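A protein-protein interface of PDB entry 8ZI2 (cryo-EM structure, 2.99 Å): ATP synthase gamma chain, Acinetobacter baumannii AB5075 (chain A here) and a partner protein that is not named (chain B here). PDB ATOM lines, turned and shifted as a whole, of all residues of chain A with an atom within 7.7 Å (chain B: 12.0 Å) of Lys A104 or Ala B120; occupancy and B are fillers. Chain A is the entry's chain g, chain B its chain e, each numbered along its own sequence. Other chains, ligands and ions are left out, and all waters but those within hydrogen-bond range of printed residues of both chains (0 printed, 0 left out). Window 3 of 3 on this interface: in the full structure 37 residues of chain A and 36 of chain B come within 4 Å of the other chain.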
ATOM      1  N   LYS A  97     -24.804   0.527 -34.949  1.00  0.00           N
ATOM      2  CA  LYS A  97     -25.695   0.699 -33.807  1.00  0.00           C
ATOM      3  C   LYS A  97     -25.200  -0.090 -32.603  1.00  0.00           C
ATOM      4  O   LYS A  97     -25.138   0.436 -31.485  1.00  0.00           O
ATOM      5  CB  LYS A  97     -27.117   0.278 -34.180  1.00  0.00           C
ATOM      6  CG  LYS A  97     -27.785   1.191 -35.190  1.00  0.00           C
ATOM      7  CD  LYS A  97     -29.255   0.846 -35.346  1.00  0.00           C
ATOM      8  CE  LYS A  97     -29.436  -0.509 -36.006  1.00  0.00           C
ATOM      9  NZ  LYS A  97     -30.867  -0.810 -36.275  1.00  0.00           N
ATOM     10  N   LYS A  98     -24.834  -1.356 -32.811  1.00  0.00           N
ATOM     11  CA  LYS A  98     -24.374  -2.154 -31.680  1.00  0.00           C
ATOM     12  C   LYS A  98     -23.073  -1.605 -31.101  1.00  0.00           C
ATOM     13  O   LYS A  98     -22.920  -1.507 -29.874  1.00  0.00           O
ATOM     14  CB  LYS A  98     -24.194  -3.613 -32.087  1.00  0.00           C
ATOM     15  CG  LYS A  98     -23.787  -4.495 -30.923  1.00  0.00           C
ATOM     16  CD  LYS A  98     -23.663  -5.939 -31.342  1.00  0.00           C
ATOM     17  CE  LYS A  98     -23.232  -6.792 -30.168  1.00  0.00           C
ATOM     18  NZ  LYS A  98     -23.102  -8.221 -30.552  1.00  0.00           N
ATOM     19  N   VAL A  99     -22.125  -1.237 -31.967  1.00  0.00           N
ATOM     20  CA  VAL A  99     -20.854  -0.736 -31.461  1.00  0.00           C
ATOM     21  C   VAL A  99     -21.039   0.607 -30.769  1.00  0.00           C
ATOM     22  O   VAL A  99     -20.365   0.888 -29.774  1.00  0.00           O
ATOM     23  CB  VAL A  99     -19.800  -0.668 -32.584  1.00  0.00           C
ATOM     24  CG1 VAL A  99     -20.090   0.465 -33.550  1.00  0.00           C
ATOM     25  CG2 VAL A  99     -18.408  -0.520 -31.990  1.00  0.00           C
ATOM     26  N   VAL A 100     -21.950   1.453 -31.257  1.00  0.00           N
ATOM     27  CA  VAL A 100     -22.153   2.736 -30.599  1.00  0.00           C
ATOM     28  C   VAL A 100     -22.844   2.536 -29.261  1.00  0.00           C
ATOM     29  O   VAL A 100     -22.560   3.258 -28.303  1.00  0.00           O
ATOM     30  CB  VAL A 100     -22.915   3.725 -31.506  1.00  0.00           C
ATOM     31  CG1 VAL A 100     -24.410   3.451 -31.512  1.00  0.00           C
ATOM     32  CG2 VAL A 100     -22.635   5.157 -31.074  1.00  0.00           C
ATOM     33  N   GLN A 101     -23.732   1.546 -29.151  1.00  0.00           N
ATOM     34  CA  GLN A 101     -24.318   1.242 -27.851  1.00  0.00           C
ATOM     35  C   GLN A 101     -23.247   0.786 -26.867  1.00  0.00           C
ATOM     36  O   GLN A 101     -23.214   1.233 -25.714  1.00  0.00           O
ATOM     37  CB  GLN A 101     -25.411   0.183 -27.998  1.00  0.00           C
ATOM     38  CG  GLN A 101     -26.676   0.698 -28.658  1.00  0.00           C
ATOM     39  CD  GLN A 101     -27.455  -0.400 -29.350  1.00  0.00           C
ATOM     40  OE1 GLN A 101     -27.058  -1.563 -29.331  1.00  0.00           O
ATOM     41  NE2 GLN A 101     -28.571  -0.034 -29.970  1.00  0.00           N
ATOM     42  N   HIS A 102     -22.346  -0.091 -27.316  1.00  0.00           N
ATOM     43  CA  HIS A 102     -21.286  -0.560 -26.425  1.00  0.00           C
ATOM     44  C   HIS A 102     -20.347   0.573 -26.020  1.00  0.00           C
ATOM     45  O   HIS A 102     -19.990   0.703 -24.840  1.00  0.00           O
ATOM     46  CB  HIS A 102     -20.507  -1.697 -27.083  1.00  0.00           C
ATOM     47  CG  HIS A 102     -21.277  -2.976 -27.180  1.00  0.00           C
ATOM     48  ND1 HIS A 102     -22.580  -3.030 -27.625  1.00  0.00           N
ATOM     49  CD2 HIS A 102     -20.927  -4.250 -26.883  1.00  0.00           C
ATOM     50  CE1 HIS A 102     -22.999  -4.283 -27.600  1.00  0.00           C
ATOM     51  NE2 HIS A 102     -22.015  -5.042 -27.154  1.00  0.00           N
ATOM     52  N   VAL A 103     -19.939   1.411 -26.975  1.00  0.00           N
ATOM     53  CA  VAL A 103     -19.024   2.494 -26.635  1.00  0.00           C
ATOM     54  C   VAL A 103     -19.719   3.537 -25.774  1.00  0.00           C
ATOM     55  O   VAL A 103     -19.080   4.167 -24.930  1.00  0.00           O
ATOM     56  CB  VAL A 103     -18.402   3.128 -27.894  1.00  0.00           C
ATOM     57  CG1 VAL A 103     -17.704   2.077 -28.737  1.00  0.00           C
ATOM     58  CG2 VAL A 103     -19.436   3.883 -28.703  1.00  0.00           C
ATOM     59  N   LYS A 104     -21.027   3.738 -25.953  1.00  0.00           N
ATOM     60  CA  LYS A 104     -21.754   4.665 -25.094  1.00  0.00           C
ATOM     61  C   LYS A 104     -21.861   4.121 -23.677  1.00  0.00           C
ATOM     62  O   LYS A 104     -21.769   4.879 -22.706  1.00  0.00           O
ATOM     63  CB  LYS A 104     -23.137   4.942 -25.681  1.00  0.00           C
ATOM     64  CG  LYS A 104     -24.016   5.829 -24.826  1.00  0.00           C
ATOM     65  CD  LYS A 104     -25.408   5.950 -25.417  1.00  0.00           C
ATOM     66  CE  LYS A 104     -26.307   6.788 -24.529  1.00  0.00           C
ATOM     67  NZ  LYS A 104     -27.694   6.858 -25.061  1.00  0.00           N
ATOM     68  N   ALA A 105     -22.042   2.806 -23.541  1.00  0.00           N
ATOM     69  CA  ALA A 105     -21.977   2.194 -22.218  1.00  0.00           C
ATOM     70  C   ALA A 105     -20.609   2.419 -21.588  1.00  0.00           C
ATOM     71  O   ALA A 105     -20.506   2.727 -20.395  1.00  0.00           O
ATOM     72  CB  ALA A 105     -22.287   0.702 -22.312  1.00  0.00           C
ATOM     73  N   GLN A 106     -19.546   2.279 -22.382  1.00  0.00           N
ATOM     74  CA  GLN A 106     -18.204   2.538 -21.867  1.00  0.00           C
ATOM     75  C   GLN A 106     -18.034   3.999 -21.461  1.00  0.00           C
ATOM     76  O   GLN A 106     -17.375   4.301 -20.458  1.00  0.00           O
ATOM     77  CB  GLN A 106     -17.156   2.142 -22.905  1.00  0.00           C
ATOM     78  CG  GLN A 106     -15.769   1.958 -22.322  1.00  0.00           C
ATOM     79  CD  GLN A 106     -15.776   1.082 -21.084  1.00  0.00           C
ATOM     80  OE1 GLN A 106     -15.356   1.505 -20.008  1.00  0.00           O
ATOM     81  NE2 GLN A 106     -16.260  -0.146 -21.232  1.00  0.00           N
ATOM     82  N   GLN A 107     -18.607   4.920 -22.239  1.00  0.00           N
ATOM     83  CA  GLN A 107     -18.573   6.337 -21.883  1.00  0.00           C
ATOM     84  C   GLN A 107     -19.267   6.578 -20.551  1.00  0.00           C
ATOM     85  O   GLN A 107     -18.763   7.316 -19.696  1.00  0.00           O
ATOM     86  CB  GLN A 107     -19.230   7.176 -22.981  1.00  0.00           C
ATOM     87  CG  GLN A 107     -18.582   7.078 -24.348  1.00  0.00           C
ATOM     88  CD  GLN A 107     -17.641   8.226 -24.632  1.00  0.00           C
ATOM     89  OE1 GLN A 107     -16.512   8.023 -25.073  1.00  0.00           O
ATOM     90  NE2 GLN A 107     -18.104   9.445 -24.389  1.00  0.00           N
ATOM     91  N   GLU A 108     -20.437   5.964 -20.360  1.00  0.00           N
ATOM     92  CA  GLU A 108     -21.116   6.055 -19.071  1.00  0.00           C
ATOM     93  C   GLU A 108     -20.314   5.389 -17.962  1.00  0.00           C
ATOM     94  O   GLU A 108     -20.500   5.727 -16.788  1.00  0.00           O
ATOM     95  CB  GLU A 108     -22.515   5.441 -19.153  1.00  0.00           C
ATOM     96  CG  GLU A 108     -23.328   5.555 -17.872  1.00  0.00           C
ATOM     97  CD  GLU A 108     -24.724   4.977 -18.013  1.00  0.00           C
ATOM     98  OE1 GLU A 108     -25.049   4.452 -19.098  1.00  0.00           O
ATOM     99  OE2 GLU A 108     -25.496   5.047 -17.034  1.00  0.00           O
ATOM    100  N   GLN A 109     -19.430   4.456 -18.306  1.00  0.00           N
ATOM    101  CA  GLN A 109     -18.470   3.914 -17.353  1.00  0.00           C
ATOM    102  C   GLN A 109     -17.258   4.819 -17.167  1.00  0.00           C
ATOM    103  O   GLN A 109     -16.292   4.403 -16.518  1.00  0.00           O
ATOM    104  CB  GLN A 109     -18.014   2.520 -17.791  1.00  0.00           C
ATOM    105  CG  GLN A 109     -19.118   1.482 -17.780  1.00  0.00           C
ATOM    106  CD  GLN A 109     -19.948   1.537 -16.515  1.00  0.00           C
ATOM    107  OE1 GLN A 109     -19.453   1.262 -15.422  1.00  0.00           O
ATOM    108  NE2 GLN A 109     -21.217   1.904 -16.654  1.00  0.00           N
ATOM    109  N   SER A 110     -17.295   6.030 -17.732  1.00  0.00           N
ATOM    110  CA  SER A 110     -16.244   7.040 -17.590  1.00  0.00           C
ATOM    111  C   SER A 110     -14.956   6.649 -18.309  1.00  0.00           C
ATOM    112  O   SER A 110     -13.860   6.953 -17.837  1.00  0.00           O
ATOM    113  CB  SER A 110     -15.953   7.352 -16.118  1.00  0.00           C
ATOM    114  OG  SER A 110     -14.864   8.249 -15.998  1.00  0.00           O
ATOM    115  N   ILE A 111     -15.071   5.974 -19.451  1.00  0.00           N
ATOM    116  CA  ILE A 111     -13.933   5.681 -20.317  1.00  0.00           C
ATOM    117  C   ILE A 111     -14.319   6.030 -21.747  1.00  0.00           C
ATOM    118  O   ILE A 111     -15.317   5.517 -22.270  1.00  0.00           O
ATOM    119  CB  ILE A 111     -13.484   4.215 -20.208  1.00  0.00           C
ATOM    120  CG1 ILE A 111     -12.717   3.984 -18.903  1.00  0.00           C
ATOM    121  CG2 ILE A 111     -12.625   3.826 -21.399  1.00  0.00           C
ATOM    122  CD1 ILE A 111     -13.564   3.459 -17.773  1.00  0.00           C
ATOM    123  N   VAL A 113     -13.489   6.170 -25.939  1.00  0.00           N
ATOM    124  CA  VAL A 113     -13.084   5.121 -26.864  1.00  0.00           C
ATOM    125  C   VAL A 113     -12.488   5.731 -28.124  1.00  0.00           C
ATOM    126  O   VAL A 113     -12.758   6.884 -28.476  1.00  0.00           O
ATOM    127  CB  VAL A 113     -14.258   4.187 -27.232  1.00  0.00           C
ATOM    128  CG1 VAL A 113     -14.910   3.621 -25.979  1.00  0.00           C
ATOM    129  CG2 VAL A 113     -15.270   4.921 -28.088  1.00  0.00           C
ATOM    130  N   TYR A 129     -20.752  12.402 -37.850  1.00  0.00           N
ATOM    131  CA  TYR A 129     -21.123  12.693 -36.475  1.00  0.00           C
ATOM    132  C   TYR A 129     -19.912  12.850 -35.566  1.00  0.00           C
ATOM    133  O   TYR A 129     -20.083  13.111 -34.371  1.00  0.00           O
ATOM    134  CB  TYR A 129     -22.038  11.593 -35.929  1.00  0.00           C
ATOM    135  CG  TYR A 129     -23.407  11.578 -36.563  1.00  0.00           C
ATOM    136  CD1 TYR A 129     -23.585  11.139 -37.867  1.00  0.00           C
ATOM    137  CD2 TYR A 129     -24.520  12.008 -35.861  1.00  0.00           C
ATOM    138  CE1 TYR A 129     -24.835  11.126 -38.453  1.00  0.00           C
ATOM    139  CE2 TYR A 129     -25.774  12.000 -36.440  1.00  0.00           C
ATOM    140  CZ  TYR A 129     -25.927  11.558 -37.735  1.00  0.00           C
ATOM    141  OH  TYR A 129     -27.176  11.549 -38.311  1.00  0.00           O
ATOM    142  N   ASP B 113     -13.637  15.094 -33.190  1.00  0.00           N
ATOM    143  CA  ASP B 113     -14.448  15.227 -31.983  1.00  0.00           C
ATOM    144  C   ASP B 113     -14.213  14.005 -31.104  1.00  0.00           C
ATOM    145  O   ASP B 113     -14.683  12.906 -31.404  1.00  0.00           O
ATOM    146  CB  ASP B 113     -15.920  15.380 -32.345  1.00  0.00           C
ATOM    147  CG  ASP B 113     -16.837  15.090 -31.180  1.00  0.00           C
ATOM    148  OD1 ASP B 113     -17.045  15.994 -30.344  1.00  0.00           O
ATOM    149  OD2 ASP B 113     -17.350  13.957 -31.099  1.00  0.00           O
ATOM    150  N   SER B 114     -13.475  14.198 -30.009  1.00  0.00           N
ATOM    151  CA  SER B 114     -13.104  13.081 -29.148  1.00  0.00           C
ATOM    152  C   SER B 114     -14.310  12.426 -28.491  1.00  0.00           C
ATOM    153  O   SER B 114     -14.226  11.256 -28.098  1.00  0.00           O
ATOM    154  CB  SER B 114     -12.121  13.553 -28.075  1.00  0.00           C
ATOM    155  OG  SER B 114     -11.871  12.532 -27.126  1.00  0.00           O
ATOM    156  N   ALA B 115     -15.421  13.146 -28.355  1.00  0.00           N
ATOM    157  CA  ALA B 115     -16.610  12.573 -27.742  1.00  0.00           C
ATOM    158  C   ALA B 115     -17.150  11.428 -28.590  1.00  0.00           C
ATOM    159  O   ALA B 115     -17.298  11.554 -29.808  1.00  0.00           O
ATOM    160  CB  ALA B 115     -17.680  13.650 -27.560  1.00  0.00           C
ATOM    161  N   ALA B 116     -17.445  10.307 -27.939  1.00  0.00           N
ATOM    162  CA  ALA B 116     -18.015   9.146 -28.610  1.00  0.00           C
ATOM    163  C   ALA B 116     -19.508   9.004 -28.385  1.00  0.00           C
ATOM    164  O   ALA B 116     -20.252   8.773 -29.342  1.00  0.00           O
ATOM    165  CB  ALA B 116     -17.314   7.866 -28.147  1.00  0.00           C
ATOM    166  N   ALA B 117     -19.970   9.141 -27.144  1.00  0.00           N
ATOM    167  CA  ALA B 117     -21.400   9.126 -26.873  1.00  0.00           C
ATOM    168  C   ALA B 117     -21.871  10.566 -27.008  1.00  0.00           C
ATOM    169  O   ALA B 117     -22.352  11.166 -26.040  1.00  0.00           O
ATOM    170  CB  ALA B 117     -21.683   8.594 -25.467  1.00  0.00           C
ATOM    171  N   LEU B 118     -21.741  11.127 -28.207  1.00  0.00           N
ATOM    172  CA  LEU B 118     -22.188  12.481 -28.487  1.00  0.00           C
ATOM    173  C   LEU B 118     -23.460  12.349 -29.311  1.00  0.00           C
ATOM    174  O   LEU B 118     -23.528  11.537 -30.240  1.00  0.00           O
ATOM    175  CB  LEU B 118     -21.154  13.323 -29.244  1.00  0.00           C
ATOM    176  CG  LEU B 118     -21.055  13.193 -30.768  1.00  0.00           C
ATOM    177  CD1 LEU B 118     -20.485  14.460 -31.385  1.00  0.00           C
ATOM    178  CD2 LEU B 118     -20.230  11.978 -31.165  1.00  0.00           C
ATOM    179  N   ALA B 119     -24.471  13.130 -28.940  1.00  0.00           N
ATOM    180  CA  ALA B 119     -25.751  13.155 -29.638  1.00  0.00           C
ATOM    181  C   ALA B 119     -26.259  11.742 -29.898  1.00  0.00           C
ATOM    182  O   ALA B 119     -26.586  11.366 -31.024  1.00  0.00           O
ATOM    183  CB  ALA B 119     -25.645  13.948 -30.939  1.00  0.00           C
ATOM    184  N   ALA B 120     -26.305  10.940 -28.830  1.00  0.00           N
ATOM    185  CA  ALA B 120     -26.784   9.568 -28.963  1.00  0.00           C
ATOM    186  C   ALA B 120     -28.194   9.531 -29.533  1.00  0.00           C
ATOM    187  O   ALA B 120     -28.576   8.555 -30.189  1.00  0.00           O
ATOM    188  CB  ALA B 120     -26.733   8.857 -27.611  1.00  0.00           C
ATOM    189  N   LEU B 121     -28.973  10.589 -29.308  1.00  0.00           N
ATOM    190  CA  LEU B 121     -30.258  10.721 -29.974  1.00  0.00           C
ATOM    191  C   LEU B 121     -30.103  10.903 -31.479  1.00  0.00           C
ATOM    192  O   LEU B 121     -30.994  10.508 -32.230  1.00  0.00           O
ATOM    193  CB  LEU B 121     -31.045  11.886 -29.370  1.00  0.00           C
ATOM    194  CG  LEU B 121     -32.555  11.914 -29.618  1.00  0.00           C
ATOM    195  CD1 LEU B 121     -33.278  12.445 -28.391  1.00  0.00           C
ATOM    196  CD2 LEU B 121     -32.893  12.754 -30.839  1.00  0.00           C
ATOM    197  N   ALA B 122     -28.987  11.464 -31.943  1.00  0.00           N
ATOM    198  CA  ALA B 122     -28.768  11.551 -33.385  1.00  0.00           C
ATOM    199  C   ALA B 122     -28.423  10.189 -33.980  1.00  0.00           C
ATOM    200  O   ALA B 122     -28.833   9.869 -35.102  1.00  0.00           O
ATOM    201  CB  ALA B 122     -27.672  12.573 -33.689  1.00  0.00           C
ATOM    202  N   GLU B 123     -27.674   9.367 -33.242  1.00  0.00           N
ATOM    203  CA  GLU B 123     -27.479   7.988 -33.672  1.00  0.00           C
ATOM    204  C   GLU B 123     -28.796   7.225 -33.657  1.00  0.00           C
ATOM    205  O   GLU B 123     -29.056   6.398 -34.537  1.00  0.00           O
ATOM    206  CB  GLU B 123     -26.435   7.304 -32.790  1.00  0.00           C
ATOM    207  CG  GLU B 123     -25.009   7.470 -33.300  1.00  0.00           C
ATOM    208  CD  GLU B 123     -24.347   8.733 -32.789  1.00  0.00           C
ATOM    209  OE1 GLU B 123     -24.919   9.386 -31.894  1.00  0.00           O
ATOM    210  OE2 GLU B 123     -23.255   9.078 -33.289  1.00  0.00           O
ATOM    211  N   THR B 124     -29.652   7.501 -32.673  1.00  0.00           N
ATOM    212  CA  THR B 124     -30.989   6.919 -32.686  1.00  0.00           C
ATOM    213  C   THR B 124     -31.820   7.455 -33.848  1.00  0.00           C
ATOM    214  O   THR B 124     -32.726   6.771 -34.329  1.00  0.00           O
ATOM    215  CB  THR B 124     -31.692   7.186 -31.355  1.00  0.00           C
ATOM    216  OG1 THR B 124     -30.729   7.159 -30.294  1.00  0.00           O
ATOM    217  CG2 THR B 124     -32.747   6.125 -31.094  1.00  0.00           C
ATOM    218  N   ALA B 125     -31.532   8.673 -34.306  1.00  0.00           N
ATOM    219  CA  ALA B 125     -32.187   9.194 -35.503  1.00  0.00           C
ATOM    220  C   ALA B 125     -31.733   8.443 -36.748  1.00  0.00           C
ATOM    221  O   ALA B 125     -32.539   8.153 -37.639  1.00  0.00           O
ATOM    222  CB  ALA B 125     -31.909  10.690 -35.646  1.00  0.00           C
ATOM    223  N   ALA B 126     -30.442   8.125 -36.828  1.00  0.00           N
ATOM    224  CA  ALA B 126     -29.972   7.242 -37.894  1.00  0.00           C
ATOM    225  C   ALA B 126     -30.648   5.878 -37.800  1.00  0.00           C
ATOM    226  O   ALA B 126     -31.015   5.276 -38.818  1.00  0.00           O
ATOM    227  CB  ALA B 126     -28.453   7.099 -37.829  1.00  0.00           C
ATOM    228  N   GLN B 127     -30.830   5.384 -36.577  1.00  0.00           N
ATOM    229  CA  GLN B 127     -31.547   4.132 -36.364  1.00  0.00           C
ATOM    230  C   GLN B 127     -32.990   4.216 -36.849  1.00  0.00           C
ATOM    231  O   GLN B 127     -33.492   3.274 -37.469  1.00  0.00           O
ATOM    232  CB  GLN B 127     -31.501   3.766 -34.880  1.00  0.00           C
ATOM    233  CG  GLN B 127     -32.575   2.795 -34.427  1.00  0.00           C
ATOM    234  CD  GLN B 127     -32.558   2.578 -32.929  1.00  0.00           C
ATOM    235  OE1 GLN B 127     -31.668   3.063 -32.231  1.00  0.00           O
ATOM    236  NE2 GLN B 127     -33.548   1.850 -32.425  1.00  0.00           N
ATOM    237  N   LEU B 128     -33.674   5.330 -36.575  1.00  0.00           N
ATOM    238  CA  LEU B 128     -35.058   5.480 -37.013  1.00  0.00           C
ATOM    239  C   LEU B 128     -35.134   5.616 -38.529  1.00  0.00           C
ATOM    240  O   LEU B 128     -36.106   5.175 -39.154  1.00  0.00           O
ATOM    241  CB  LEU B 128     -35.713   6.674 -36.307  1.00  0.00           C
ATOM    242  CG  LEU B 128     -35.503   8.143 -36.705  1.00  0.00           C
ATOM    243  CD1 LEU B 128     -36.314   8.567 -37.927  1.00  0.00           C
ATOM    244  CD2 LEU B 128     -35.819   9.051 -35.525  1.00  0.00           C
ATOM    245  N   GLU B 129     -34.120   6.236 -39.136  1.00  0.00           N
ATOM    246  CA  GLU B 129     -34.016   6.225 -40.590  1.00  0.00           C
ATOM    247  C   GLU B 129     -33.894   4.798 -41.106  1.00  0.00           C
ATOM    248  O   GLU B 129     -34.541   4.429 -42.092  1.00  0.00           O
ATOM    249  CB  GLU B 129     -32.812   7.059 -41.034  1.00  0.00           C
ATOM    250  CG  GLU B 129     -32.419   6.997 -42.523  1.00  0.00           C
ATOM    251  CD  GLU B 129     -33.554   7.310 -43.500  1.00  0.00           C
ATOM    252  OE1 GLU B 129     -34.568   6.584 -43.551  1.00  0.00           O
ATOM    253  OE2 GLU B 129     -33.424   8.310 -44.235  1.00  0.00           O
ATOM    254  N   THR B 130     -33.084   3.977 -40.436  1.00  0.00           N
ATOM    255  CA  THR B 130     -33.024   2.559 -40.780  1.00  0.00           C
ATOM    256  C   THR B 130     -34.390   1.902 -40.621  1.00  0.00           C
ATOM    257  O   THR B 130     -34.755   1.009 -41.393  1.00  0.00           O
ATOM    258  CB  THR B 130     -31.985   1.853 -39.913  1.00  0.00           C
ATOM    259  OG1 THR B 130     -30.785   2.633 -39.887  1.00  0.00           O
ATOM    260  CG2 THR B 130     -31.676   0.471 -40.473  1.00  0.00           C
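O of Ala B120 sits at hydrogen-bond distance from OG1 of Thr B124 (2.6 Å). The backbone carbonyl oxygen (O) of Ala B119 sits close to the side-chain carboxylate (OE1) of Glu B123, at 2.7 Å.
The side-chain amide nitrogen (NE2) of Gln A107 lies close to the backbone NH (N) of Ala B117 (3.3 Å).
Lys A97 touches Gln B127 (CD to CB, 3.7 Å). Glu B123 touches Val A100. CG of Lys A104 touches CB of Ala B117 (3.7 Å). CB of Ala B120 touches NZ of Lys A104, 3.4 Å away. Ala B116 touches Gln A107 (CB to OE1, 3.2 Å). CG2 of Val A113 touches CB of Ala B116, at 3.6 Å. Tyr A129 touches Leu B118. Tyr A129 touches Ala B122 (CE2 to CB, 3.4 Å). CB of Tyr A129 touches OE2 of Glu B123, 3.8 Å away.
Printed residues of chain B within 4 Å of Val A100: Glu B123. His A102 touches none of the printed residues of chain B. Of chain B, only Ala B117 (3.7 Å) and Ala B120 (3.4 Å) come within 4 Å of Lys A104. No residue of chain B comes within 4 Å of Ala A105. No residue of chain B comes within 4 Å of Gln A106. Of chain B, only Ala B116 (3.2 Å) and Ala B117 (3.3 Å) come within 4 Å of Gln A107. Glu A108 touches none of the printed residues of chain B. Of the printed residues of chain B, Val A113 touches Ala B116 (3.6 Å). Of the printed residues of chain A, Leu B118 touches Tyr A129. Printed residues of chain A within 4 Å of Ala B120: Lys A104. Of the printed residues of chain A, Ala B122 touches Tyr A129. Ala B126 touches none of the printed residues of chain A. The nearest printed residue of chain B that does not touch Lys A97 is Thr B130 (4.5 Å).
Of the 17 printed residues of chain A, 6 touch a printed residue of chain B. Printed residues of chain B that touch a printed residue of chain A: Ala B116, Ala B117, Leu B118, Ala B120, Ala B122, Glu B123 and Gln B127. Among the printed residues, 10 pairs touch across the chains.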
